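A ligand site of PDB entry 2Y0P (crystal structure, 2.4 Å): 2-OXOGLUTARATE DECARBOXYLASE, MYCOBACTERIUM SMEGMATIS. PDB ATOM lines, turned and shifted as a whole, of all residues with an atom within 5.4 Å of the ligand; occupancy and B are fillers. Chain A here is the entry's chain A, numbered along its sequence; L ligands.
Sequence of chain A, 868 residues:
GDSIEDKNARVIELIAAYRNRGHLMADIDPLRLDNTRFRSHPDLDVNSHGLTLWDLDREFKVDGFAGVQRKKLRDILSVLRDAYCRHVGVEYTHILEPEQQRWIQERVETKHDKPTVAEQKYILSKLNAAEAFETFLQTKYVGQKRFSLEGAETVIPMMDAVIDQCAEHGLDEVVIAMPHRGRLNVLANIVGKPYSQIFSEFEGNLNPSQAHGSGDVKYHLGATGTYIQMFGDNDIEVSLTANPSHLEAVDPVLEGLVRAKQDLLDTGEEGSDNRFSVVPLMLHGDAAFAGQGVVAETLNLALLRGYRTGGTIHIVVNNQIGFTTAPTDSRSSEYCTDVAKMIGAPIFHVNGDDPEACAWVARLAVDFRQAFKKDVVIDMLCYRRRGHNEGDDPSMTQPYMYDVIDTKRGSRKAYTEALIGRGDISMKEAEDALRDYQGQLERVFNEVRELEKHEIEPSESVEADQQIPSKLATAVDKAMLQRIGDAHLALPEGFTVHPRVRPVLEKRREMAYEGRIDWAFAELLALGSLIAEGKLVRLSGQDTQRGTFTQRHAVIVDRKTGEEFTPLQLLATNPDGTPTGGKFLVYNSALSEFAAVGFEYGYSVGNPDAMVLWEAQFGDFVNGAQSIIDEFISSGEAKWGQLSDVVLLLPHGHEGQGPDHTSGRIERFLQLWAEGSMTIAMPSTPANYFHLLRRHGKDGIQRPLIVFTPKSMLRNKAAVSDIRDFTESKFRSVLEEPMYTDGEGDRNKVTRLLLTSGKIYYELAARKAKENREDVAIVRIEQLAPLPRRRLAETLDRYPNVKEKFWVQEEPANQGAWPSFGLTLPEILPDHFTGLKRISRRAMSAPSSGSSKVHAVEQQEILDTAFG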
ATOM      1  N   GLU A 463      18.626  -5.888  17.907  1.00  0.00           N
ATOM      2  CA  GLU A 463      17.861  -5.048  18.846  1.00  0.00           C
ATOM      3  C   GLU A 463      16.432  -4.709  18.352  1.00  0.00           C
ATOM      4  O   GLU A 463      15.472  -4.913  19.102  1.00  0.00           O
ATOM      5  CB  GLU A 463      18.634  -3.740  19.167  1.00  0.00           C
ATOM      6  CG  GLU A 463      18.048  -2.936  20.320  1.00  0.00           C
ATOM      7  CD  GLU A 463      18.979  -2.050  21.138  1.00  0.00           C
ATOM      8  OE1 GLU A 463      20.128  -1.812  20.706  1.00  0.00           O
ATOM      9  OE2 GLU A 463      18.548  -1.600  22.223  1.00  0.00           O
ATOM     10  N   GLN A 466      12.721  -7.139  18.166  1.00  0.00           N
ATOM     11  CA  GLN A 466      11.699  -7.183  19.209  1.00  0.00           C
ATOM     12  C   GLN A 466      11.398  -5.753  19.643  1.00  0.00           C
ATOM     13  O   GLN A 466      12.258  -5.083  20.248  1.00  0.00           O
ATOM     14  CB  GLN A 466      12.159  -8.066  20.392  1.00  0.00           C
ATOM     15  CG  GLN A 466      12.579  -9.477  19.966  1.00  0.00           C
ATOM     16  CD  GLN A 466      11.822 -10.579  20.674  1.00  0.00           C
ATOM     17  OE1 GLN A 466      10.582 -10.608  20.693  1.00  0.00           O
ATOM     18  NE2 GLN A 466      12.561 -11.521  21.239  1.00  0.00           N
ATOM     19  N   ILE A 468       9.262  -2.758  21.641  1.00  0.00           N
ATOM     20  CA  ILE A 468       8.576  -2.446  22.900  1.00  0.00           C
ATOM     21  C   ILE A 468       7.110  -2.066  22.570  1.00  0.00           C
ATOM     22  O   ILE A 468       6.890  -1.206  21.714  1.00  0.00           O
ATOM     23  CB  ILE A 468       9.324  -1.329  23.693  1.00  0.00           C
ATOM     24  CG1 ILE A 468      10.659  -1.853  24.250  1.00  0.00           C
ATOM     25  CG2 ILE A 468       8.449  -0.725  24.810  1.00  0.00           C
ATOM     26  CD1 ILE A 468      11.684  -0.762  24.597  1.00  0.00           C
ATOM     27  N   PRO A 469       6.100  -2.710  23.210  1.00  0.00           N
ATOM     28  CA  PRO A 469       4.712  -2.329  22.912  1.00  0.00           C
ATOM     29  C   PRO A 469       4.363  -0.948  23.482  1.00  0.00           C
ATOM     30  O   PRO A 469       4.912  -0.538  24.510  1.00  0.00           O
ATOM     31  CB  PRO A 469       3.897  -3.451  23.558  1.00  0.00           C
ATOM     32  CG  PRO A 469       4.748  -3.938  24.655  1.00  0.00           C
ATOM     33  CD  PRO A 469       6.178  -3.770  24.229  1.00  0.00           C
ATOM     34  N   SER A 470       3.465  -0.224  22.805  1.00  0.00           N
ATOM     35  CA  SER A 470       3.031   1.118  23.193  1.00  0.00           C
ATOM     36  C   SER A 470       1.930   1.056  24.244  1.00  0.00           C
ATOM     37  O   SER A 470       0.995   0.248  24.117  1.00  0.00           O
ATOM     38  CB  SER A 470       2.542   1.887  21.972  1.00  0.00           C
ATOM     39  N   LYS A 471       2.037   1.916  25.276  1.00  0.00           N
ATOM     40  CA  LYS A 471       1.091   2.109  26.390  1.00  0.00           C
ATOM     41  C   LYS A 471       0.635   0.775  27.023  1.00  0.00           C
ATOM     42  O   LYS A 471      -0.555   0.470  27.039  1.00  0.00           O
ATOM     43  CB  LYS A 471      -0.129   2.944  25.915  1.00  0.00           C
ATOM     44  CG  LYS A 471       0.187   4.404  25.600  1.00  0.00           C
ATOM     45  CD  LYS A 471      -0.035   5.295  26.815  1.00  0.00           C
ATOM     46  CE  LYS A 471       0.832   6.530  26.780  1.00  0.00           C
ATOM     47  NZ  LYS A 471       0.524   7.435  27.909  1.00  0.00           N
ATOM     48  N   LEU A 472       1.604  -0.013  27.548  1.00  0.00           N
ATOM     49  CA  LEU A 472       1.301  -1.291  28.179  1.00  0.00           C
ATOM     50  C   LEU A 472       1.025  -1.089  29.672  1.00  0.00           C
ATOM     51  O   LEU A 472       1.900  -0.610  30.411  1.00  0.00           O
ATOM     52  CB  LEU A 472       2.437  -2.315  27.956  1.00  0.00           C
ATOM     53  CG  LEU A 472       2.266  -3.679  28.605  1.00  0.00           C
ATOM     54  CD1 LEU A 472       1.519  -4.639  27.696  1.00  0.00           C
ATOM     55  CD2 LEU A 472       3.598  -4.258  28.986  1.00  0.00           C
ATOM     56  N   TRP A 673      25.938  -7.600  27.802  1.00  0.00           N
ATOM     57  CA  TRP A 673      24.833  -6.876  27.165  1.00  0.00           C
ATOM     58  C   TRP A 673      25.295  -6.161  25.903  1.00  0.00           C
ATOM     59  O   TRP A 673      26.297  -5.431  25.927  1.00  0.00           O
ATOM     60  CB  TRP A 673      24.183  -5.851  28.118  1.00  0.00           C
ATOM     61  CG  TRP A 673      22.872  -5.314  27.612  1.00  0.00           C
ATOM     62  CD1 TRP A 673      21.632  -5.769  27.937  1.00  0.00           C
ATOM     63  CD2 TRP A 673      22.672  -4.246  26.665  1.00  0.00           C
ATOM     64  NE1 TRP A 673      20.669  -5.050  27.269  1.00  0.00           N
ATOM     65  CE2 TRP A 673      21.272  -4.113  26.476  1.00  0.00           C
ATOM     66  CE3 TRP A 673      23.537  -3.380  25.962  1.00  0.00           C
ATOM     67  CZ2 TRP A 673      20.733  -3.144  25.630  1.00  0.00           C
ATOM     68  CZ3 TRP A 673      22.992  -2.460  25.075  1.00  0.00           C
ATOM     69  CH2 TRP A 673      21.611  -2.350  24.914  1.00  0.00           C
ATOM     70  N   GLY A 676      20.447  -4.899  22.631  1.00  0.00           N
ATOM     71  CA  GLY A 676      19.226  -5.017  23.436  1.00  0.00           C
ATOM     72  C   GLY A 676      18.766  -6.445  23.656  1.00  0.00           C
ATOM     73  O   GLY A 676      17.564  -6.713  23.572  1.00  0.00           O
ATOM     74  N   SER A 677      19.718  -7.368  23.913  1.00  0.00           N
ATOM     75  CA  SER A 677      19.483  -8.799  24.068  1.00  0.00           C
ATOM     76  C   SER A 677      18.725  -9.135  25.352  1.00  0.00           C
ATOM     77  O   SER A 677      17.899 -10.042  25.353  1.00  0.00           O
ATOM     78  CB  SER A 677      20.806  -9.568  24.035  1.00  0.00           C
ATOM     79  OG  SER A 677      21.719  -9.137  25.036  1.00  0.00           O
ATOM     80  N   MET A 678      19.035  -8.412  26.452  1.00  0.00           N
ATOM     81  CA  MET A 678      18.413  -8.646  27.755  1.00  0.00           C
ATOM     82  C   MET A 678      18.023  -7.349  28.442  1.00  0.00           C
ATOM     83  O   MET A 678      18.493  -6.274  28.058  1.00  0.00           O
ATOM     84  CB  MET A 678      19.385  -9.401  28.715  1.00  0.00           C
ATOM     85  CG  MET A 678      20.172 -10.530  28.098  1.00  0.00           C
ATOM     86  SD  MET A 678      21.518 -11.037  29.203  1.00  0.00           S
ATOM     87  CE  MET A 678      22.761  -9.825  28.818  1.00  0.00           C
ATOM     88  N   THR A 679      17.209  -7.458  29.504  1.00  0.00           N
ATOM     89  CA  THR A 679      16.846  -6.386  30.411  1.00  0.00           C
ATOM     90  C   THR A 679      17.613  -6.678  31.687  1.00  0.00           C
ATOM     91  O   THR A 679      17.561  -7.803  32.172  1.00  0.00           O
ATOM     92  CB  THR A 679      15.316  -6.263  30.607  1.00  0.00           C
ATOM     93  OG1 THR A 679      14.698  -5.972  29.360  1.00  0.00           O
ATOM     94  CG2 THR A 679      14.939  -5.169  31.603  1.00  0.00           C
ATOM     95  N   ARG A 695       5.557  -6.427  33.583  1.00  0.00           N
ATOM     96  CA  ARG A 695       5.880  -5.953  32.238  1.00  0.00           C
ATOM     97  C   ARG A 695       6.502  -7.093  31.430  1.00  0.00           C
ATOM     98  O   ARG A 695       6.021  -7.394  30.344  1.00  0.00           O
ATOM     99  CB  ARG A 695       6.801  -4.721  32.260  1.00  0.00           C
ATOM    100  CG  ARG A 695       6.946  -4.009  30.913  1.00  0.00           C
ATOM    101  CD  ARG A 695       7.898  -2.831  30.990  1.00  0.00           C
ATOM    102  NE  ARG A 695       9.243  -3.250  31.410  1.00  0.00           N
ATOM    103  CZ  ARG A 695      10.276  -2.431  31.540  1.00  0.00           C
ATOM    104  NH1 ARG A 695      10.136  -1.131  31.276  1.00  0.00           N
ATOM    105  NH2 ARG A 695      11.451  -2.899  31.929  1.00  0.00           N
ATOM    106  N   ASP A 699       4.599  -7.796  28.042  1.00  0.00           N
ATOM    107  CA  ASP A 699       5.097  -7.011  26.896  1.00  0.00           C
ATOM    108  C   ASP A 699       5.294  -7.825  25.607  1.00  0.00           C
ATOM    109  O   ASP A 699       5.370  -7.223  24.524  1.00  0.00           O
ATOM    110  CB  ASP A 699       6.416  -6.286  27.260  1.00  0.00           C
ATOM    111  CG  ASP A 699       7.597  -7.138  27.737  1.00  0.00           C
ATOM    112  OD1 ASP A 699       7.440  -8.381  27.832  1.00  0.00           O
ATOM    113  OD2 ASP A 699       8.646  -6.547  28.072  1.00  0.00           O
ATOM    114  N   ILE A 701       7.949  -9.542  24.729  1.00  0.00           N
ATOM    115  CA  ILE A 701       9.345  -9.471  24.313  1.00  0.00           C
ATOM    116  C   ILE A 701      10.018 -10.749  24.826  1.00  0.00           C
ATOM    117  O   ILE A 701      10.233 -10.909  26.028  1.00  0.00           O
ATOM    118  CB  ILE A 701      10.029  -8.156  24.812  1.00  0.00           C
ATOM    119  CG1 ILE A 701       9.326  -6.910  24.208  1.00  0.00           C
ATOM    120  CG2 ILE A 701      11.529  -8.147  24.498  1.00  0.00           C
ATOM    121  CD1 ILE A 701       9.587  -5.585  24.950  1.00  0.00           C
ATOM    122  N   ARG A 703      12.847 -11.998  25.416  1.00  0.00           N
ATOM    123  CA  ARG A 703      14.221 -11.626  25.750  1.00  0.00           C
ATOM    124  C   ARG A 703      14.432 -11.807  27.257  1.00  0.00           C
ATOM    125  O   ARG A 703      13.495 -11.548  28.017  1.00  0.00           O
ATOM    126  CB  ARG A 703      14.550 -10.198  25.292  1.00  0.00           C
ATOM    127  CG  ARG A 703      14.707 -10.121  23.784  1.00  0.00           C
ATOM    128  CD  ARG A 703      15.122  -8.769  23.287  1.00  0.00           C
ATOM    129  NE  ARG A 703      15.470  -8.847  21.859  1.00  0.00           N
ATOM    130  CZ  ARG A 703      15.683  -7.799  21.080  1.00  0.00           C
ATOM    131  NH1 ARG A 703      15.582  -6.560  21.554  1.00  0.00           N
ATOM    132  NH2 ARG A 703      15.975  -7.976  19.790  1.00  0.00           N
ATOM    133  N   LYS A 730       3.254   2.550  36.967  1.00  0.00           N
ATOM    134  CA  LYS A 730       3.841   1.658  35.962  1.00  0.00           C
ATOM    135  C   LYS A 730       5.313   1.477  36.312  1.00  0.00           C
ATOM    136  O   LYS A 730       5.758   2.016  37.330  1.00  0.00           O
ATOM    137  CB  LYS A 730       3.654   2.262  34.550  1.00  0.00           C
ATOM    138  N   PHE A 731       6.092   0.743  35.500  1.00  0.00           N
ATOM    139  CA  PHE A 731       7.511   0.622  35.829  1.00  0.00           C
ATOM    140  C   PHE A 731       8.219   1.960  35.586  1.00  0.00           C
ATOM    141  O   PHE A 731       7.974   2.624  34.574  1.00  0.00           O
ATOM    142  CB  PHE A 731       8.210  -0.530  35.058  1.00  0.00           C
ATOM    143  CG  PHE A 731       9.695  -0.646  35.356  1.00  0.00           C
ATOM    144  CD1 PHE A 731      10.140  -1.203  36.548  1.00  0.00           C
ATOM    145  CD2 PHE A 731      10.640  -0.148  34.468  1.00  0.00           C
ATOM    146  CE1 PHE A 731      11.502  -1.274  36.847  1.00  0.00           C
ATOM    147  CE2 PHE A 731      12.008  -0.239  34.753  1.00  0.00           C
ATOM    148  CZ  PHE A 731      12.430  -0.785  35.944  1.00  0.00           C
ATOM    149  N   SER A 733      11.949   3.403  35.307  1.00  0.00           N
ATOM    150  CA  SER A 733      13.358   3.073  35.091  1.00  0.00           C
ATOM    151  C   SER A 733      14.285   4.047  35.807  1.00  0.00           C
ATOM    152  O   SER A 733      15.388   3.671  36.200  1.00  0.00           O
ATOM    153  CB  SER A 733      13.683   3.055  33.608  1.00  0.00           C
ATOM    154  OG  SER A 733      13.283   4.268  32.993  1.00  0.00           O
ATOM    155  N   GLN A 783      16.566   0.482  35.855  1.00  0.00           N
ATOM    156  CA  GLN A 783      16.874  -0.346  34.686  1.00  0.00           C
ATOM    157  C   GLN A 783      18.259   0.026  34.200  1.00  0.00           C
ATOM    158  O   GLN A 783      18.471   1.125  33.700  1.00  0.00           O
ATOM    159  CB  GLN A 783      15.796  -0.145  33.589  1.00  0.00           C
ATOM    160  CG  GLN A 783      15.923  -1.115  32.419  1.00  0.00           C
ATOM    161  CD  GLN A 783      14.818  -0.908  31.423  1.00  0.00           C
ATOM    162  OE1 GLN A 783      13.646  -1.195  31.691  1.00  0.00           O
ATOM    163  NE2 GLN A 783      15.158  -0.379  30.259  1.00  0.00           N
ATOM    164  N   ALA A 785      20.196  -1.813  31.934  1.00  0.00           N
ATOM    165  CA  ALA A 785      20.311  -2.111  30.500  1.00  0.00           C
ATOM    166  C   ALA A 785      18.976  -2.654  29.948  1.00  0.00           C
ATOM    167  O   ALA A 785      18.421  -3.583  30.550  1.00  0.00           O
ATOM    168  CB  ALA A 785      21.448  -3.105  30.255  1.00  0.00           C
ATOM    169  N   PRO A 786      18.412  -2.123  28.840  1.00  0.00           N
ATOM    170  CA  PRO A 786      18.889  -0.975  28.032  1.00  0.00           C
ATOM    171  C   PRO A 786      18.819   0.302  28.871  1.00  0.00           C
ATOM    172  O   PRO A 786      17.950   0.418  29.747  1.00  0.00           O
ATOM    173  CB  PRO A 786      17.933  -0.971  26.829  1.00  0.00           C
ATOM    174  CG  PRO A 786      16.675  -1.571  27.349  1.00  0.00           C
ATOM    175  CD  PRO A 786      17.122  -2.630  28.327  1.00  0.00           C
ATOM    176  N   LEU A 787      19.797   1.209  28.670  1.00  0.00           N
ATOM    177  CA  LEU A 787      19.885   2.455  29.427  1.00  0.00           C
ATOM    178  C   LEU A 787      18.737   3.393  29.070  1.00  0.00           C
ATOM    179  O   LEU A 787      18.526   3.709  27.892  1.00  0.00           O
ATOM    180  CB  LEU A 787      21.232   3.171  29.188  1.00  0.00           C
ATOM    181  CG  LEU A 787      22.279   3.076  30.302  1.00  0.00           C
ATOM    182  CD1 LEU A 787      23.643   3.531  29.789  1.00  0.00           C
ATOM    183  CD2 LEU A 787      21.878   3.895  31.527  1.00  0.00           C
ATOM    184  N   PRO A 788      17.958   3.842  30.090  1.00  0.00           N
ATOM    185  CA  PRO A 788      16.848   4.764  29.790  1.00  0.00           C
ATOM    186  C   PRO A 788      17.400   6.166  29.572  1.00  0.00           C
ATOM    187  O   PRO A 788      17.284   7.031  30.440  1.00  0.00           O
ATOM    188  CB  PRO A 788      15.959   4.633  31.035  1.00  0.00           C
ATOM    189  CG  PRO A 788      16.870   4.213  32.132  1.00  0.00           C
ATOM    190  CD  PRO A 788      18.081   3.570  31.536  1.00  0.00           C
ATOM    191  N   ARG A 789      18.035   6.389  28.404  1.00  0.00           N
ATOM    192  CA  ARG A 789      18.709   7.627  28.023  1.00  0.00           C
ATOM    193  C   ARG A 789      17.776   8.845  28.065  1.00  0.00           C
ATOM    194  O   ARG A 789      18.136   9.852  28.668  1.00  0.00           O
ATOM    195  CB  ARG A 789      19.355   7.503  26.633  1.00  0.00           C
ATOM    196  CG  ARG A 789      20.400   8.582  26.340  1.00  0.00           C
ATOM    197  CD  ARG A 789      21.104   8.374  25.016  1.00  0.00           C
ATOM    198  NE  ARG A 789      20.302   8.868  23.891  1.00  0.00           N
ATOM    199  CZ  ARG A 789      20.492  10.032  23.278  1.00  0.00           C
ATOM    200  NH1 ARG A 789      21.455  10.858  23.685  1.00  0.00           N
ATOM    201  NH2 ARG A 789      19.732  10.383  22.258  1.00  0.00           N
ATOM    202  N   ARG A 790      16.580   8.734  27.445  1.00  0.00           N
ATOM    203  CA  ARG A 790      15.577   9.802  27.364  1.00  0.00           C
ATOM    204  C   ARG A 790      15.028  10.162  28.754  1.00  0.00           C
ATOM    205  O   ARG A 790      15.035  11.353  29.096  1.00  0.00           O
ATOM    206  CB  ARG A 790      14.445   9.428  26.411  1.00  0.00           C
ATOM    207  N   ARG A 791      14.596   9.157  29.562  1.00  0.00           N
ATOM    208  CA  ARG A 791      14.057   9.390  30.911  1.00  0.00           C
ATOM    209  C   ARG A 791      15.139   9.984  31.832  1.00  0.00           C
ATOM    210  O   ARG A 791      14.824  10.915  32.570  1.00  0.00           O
ATOM    211  CB  ARG A 791      13.447   8.121  31.525  1.00  0.00           C
ATOM    212  CG  ARG A 791      12.555   8.457  32.711  1.00  0.00           C
ATOM    213  CD  ARG A 791      11.855   7.284  33.355  1.00  0.00           C
ATOM    214  NE  ARG A 791      11.059   7.725  34.508  1.00  0.00           N
ATOM    215  CZ  ARG A 791       9.769   8.052  34.455  1.00  0.00           C
ATOM    216  NH1 ARG A 791       9.095   7.935  33.312  1.00  0.00           N
ATOM    217  NH2 ARG A 791       9.138   8.453  35.543  1.00  0.00           N
ATOM    218  N   LEU A 792      16.388   9.460  31.769  1.00  0.00           N
ATOM    219  CA  LEU A 792      17.500   9.942  32.583  1.00  0.00           C
ATOM    220  C   LEU A 792      17.806  11.412  32.271  1.00  0.00           C
ATOM    221  O   LEU A 792      17.889  12.203  33.216  1.00  0.00           O
ATOM    222  CB  LEU A 792      18.753   9.069  32.387  1.00  0.00           C
ATOM    223  CG  LEU A 792      19.986   9.326  33.266  1.00  0.00           C
ATOM    224  CD1 LEU A 792      19.669   9.247  34.754  1.00  0.00           C
ATOM    225  CD2 LEU A 792      21.080   8.342  32.941  1.00  0.00           C
HETATM  226  N1  LIG L   1      11.561  -3.974  28.238  1.00  0.00           N
HETATM  227  C1  LIG L   1      10.263  -3.639  28.018  1.00  0.00           C
HETATM  228  N2  LIG L   1       9.826  -2.361  27.971  1.00  0.00           N
HETATM  229  C2  LIG L   1      10.692  -1.347  28.130  1.00  0.00           C
HETATM  230  C3  LIG L   1      12.085  -1.624  28.357  1.00  0.00           C
HETATM  231  C4  LIG L   1      12.492  -3.003  28.406  1.00  0.00           C
HETATM  232  N3  LIG L   1      13.813  -3.318  28.606  1.00  0.00           N
HETATM  233  N4  LIG L   1      12.716  -0.427  28.489  1.00  0.00           N
HETATM  234  C5  LIG L   1      11.853   0.536  28.368  1.00  0.00           C
HETATM  235  N5  LIG L   1      10.598   0.012  28.139  1.00  0.00           N
HETATM  236  C6  LIG L   1       9.360   0.767  27.950  1.00  0.00           C
HETATM  237  C7  LIG L   1       8.885   1.391  29.284  1.00  0.00           C
HETATM  238  O1  LIG L   1       8.082   0.508  30.098  1.00  0.00           O
HETATM  239  C8  LIG L   1       8.109   2.649  28.782  1.00  0.00           C
HETATM  240  O2  LIG L   1       6.826   2.296  28.284  1.00  0.00           O
HETATM  241  P1  LIG L   1       5.836   3.541  28.556  1.00  0.00           P
HETATM  242  O3  LIG L   1       4.353   3.058  28.137  1.00  0.00           O
HETATM  243  O4  LIG L   1       5.855   3.980  30.107  1.00  0.00           O
HETATM  244  O5  LIG L   1       6.249   4.690  27.698  1.00  0.00           O
HETATM  245  C9  LIG L   1       8.941   3.075  27.576  1.00  0.00           C
HETATM  246  O6  LIG L   1       9.629   1.897  27.073  1.00  0.00           O
HETATM  247  C10 LIG L   1       9.858   4.217  27.996  1.00  0.00           C
HETATM  248  O7  LIG L   1      11.098   3.663  28.398  1.00  0.00           O
HETATM  249  P2  LIG L   1      11.790   4.497  29.571  1.00  0.00           P
HETATM  250  O8  LIG L   1      11.118   5.943  29.866  1.00  0.00           O
HETATM  251  O9  LIG L   1      11.700   3.733  30.822  1.00  0.00           O
HETATM  252  O10 LIG L   1      13.328   4.653  29.126  1.00  0.00           O
HETATM  253  P3  LIG L   1      13.631   5.590  27.819  1.00  0.00           P
HETATM  254  O11 LIG L   1      14.555   6.782  28.258  1.00  0.00           O
HETATM  255  O12 LIG L   1      12.442   6.100  27.110  1.00  0.00           O
HETATM  256  O13 LIG L   1      14.572   4.850  26.768  1.00  0.00           O
HETATM  257  C11 LIG L   1      14.940   2.588  26.210  1.00  0.00           C
HETATM  258  C12 LIG L   1      13.906   3.695  26.240  1.00  0.00           C
HETATM  259  C13 LIG L   1      14.310   1.446  25.430  1.00  0.00           C
HETATM  260  C14 LIG L   1      15.170   2.197  27.676  1.00  0.00           C
HETATM  261  C15 LIG L   1      16.272   3.060  25.551  1.00  0.00           C
HETATM  262  O14 LIG L   1      17.412   2.262  25.922  1.00  0.00           O
HETATM  263  C16 LIG L   1      16.159   3.253  24.047  1.00  0.00           C
HETATM  264  O15 LIG L   1      15.518   4.195  23.615  1.00  0.00           O
HETATM  265  N6  LIG L   1      16.762   2.357  23.222  1.00  0.00           N
HETATM  266  C17 LIG L   1      16.728   2.387  21.754  1.00  0.00           C
HETATM  267  C18 LIG L   1      16.848   0.956  21.222  1.00  0.00           C
HETATM  268  C19 LIG L   1      15.628   0.147  21.617  1.00  0.00           C
HETATM  269  O16 LIG L   1      14.539   0.480  21.188  1.00  0.00           O
HETATM  270  N7  LIG L   1      15.795  -0.933  22.440  1.00  0.00           N
HETATM  271  C20 LIG L   1      14.670  -1.774  22.864  1.00  0.00           C
HETATM  272  C21 LIG L   1      15.052  -2.575  24.086  1.00  0.00           C
HETATM  273  S1  LIG L   1      14.830  -4.353  23.814  1.00  0.00           S
HETATM  274  C22 LIG L   1      15.633  -4.933  25.234  1.00  0.00           C
HETATM  275  O17 LIG L   1      16.685  -4.435  25.582  1.00  0.00           O
HETATM  276  C23 LIG L   1      15.098  -6.066  26.070  1.00  0.00           C
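O14 of the ligand is in hydrogen-bond range of O of Leu 787 (2.7 Å). An oxygen (O11) of the ligand sits at hydrogen-bond distance from the backbone NH (N) of Arg 791, 2.7 Å away. OG of Ser 733 lies within hydrogen-bond range of O9 of the ligand (2.7 Å). N7 of the ligand sits at hydrogen-bond distance from OE2 of Glu 463 (2.8 Å). NH1 of Arg 695 is in hydrogen-bond range of O1 of the ligand, 2.9 Å away. OG1 of Thr 679 is in hydrogen-bond range of N3 of the ligand, at 2.9 Å. The backbone NH (N) of Arg 790 is in hydrogen-bond range of an oxygen (O11) of the ligand (2.9 Å). NE2 of Gln 783 lies within hydrogen-bond range of N4 of the ligand. The guanidinium group (NH1) of Arg 703 lies close to a sulfur (S1) of the ligand (3.2 Å).
The backbone carbonyl oxygen (O) of Ser 733 is in hydrogen-bond range of the backbone NH (N) of Gln 783, at 3.4 Å. The backbone carbonyl oxygen of Glu 463 is in hydrogen-bond range of the guanidinium group of Arg 703 (3.0 Å). The guanidinium group (NH2) of Arg 695 is in hydrogen-bond range of the side-chain amide oxygen (OE1) of Gln 783, 2.8 Å away. The side-chain amide nitrogen of Gln 783 lies within hydrogen-bond range of the backbone carbonyl oxygen of Pro 786 (2.9 Å). O of Gly 676 sits at hydrogen-bond distance from NH1 of Arg 703, at 2.8 Å. The side-chain carboxylate (OD1) of Asp 699 sits close to the backbone NH (N) of Ile 701, at 3.4 Å. NE1 of Trp 673 sits at hydrogen-bond distance from O of Met 678, 2.6 Å away.
An oxygen (O17) of the ligand lies close to the backbone carbonyl oxygen of Gly 676 (3.2 Å). CD1 of Ile 468 touches C13 of the ligand, at 3.5 Å. Lys 471 touches the ligand (CA to O3, 3.8 Å). Met 678 touches the ligand (O to O17, 3.6 Å). Asp 699 touches the ligand. CD1 of Ile 701 touches C1 of the ligand, at 3.7 Å. Pro 786 touches the ligand. C of Pro 788 touches O11 of the ligand, 3.2 Å away. Arg 789 touches the ligand (N to O11, 3.5 Å). Hydrophobic or aromatic side chains within 4 Å of the ligand: Ile 468, Ile 701, Pro 786 and Pro 788. Within 4 Å of the ligand: Glu 463, Ile 468, Lys 471, Gly 676, Met 678, Thr 679, Arg 695, Asp 699, Ile 701, Arg 703, Ser 733, Gln 783, Pro 786, Leu 787, Pro 788, Arg 789, Arg 790 and Arg 791.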
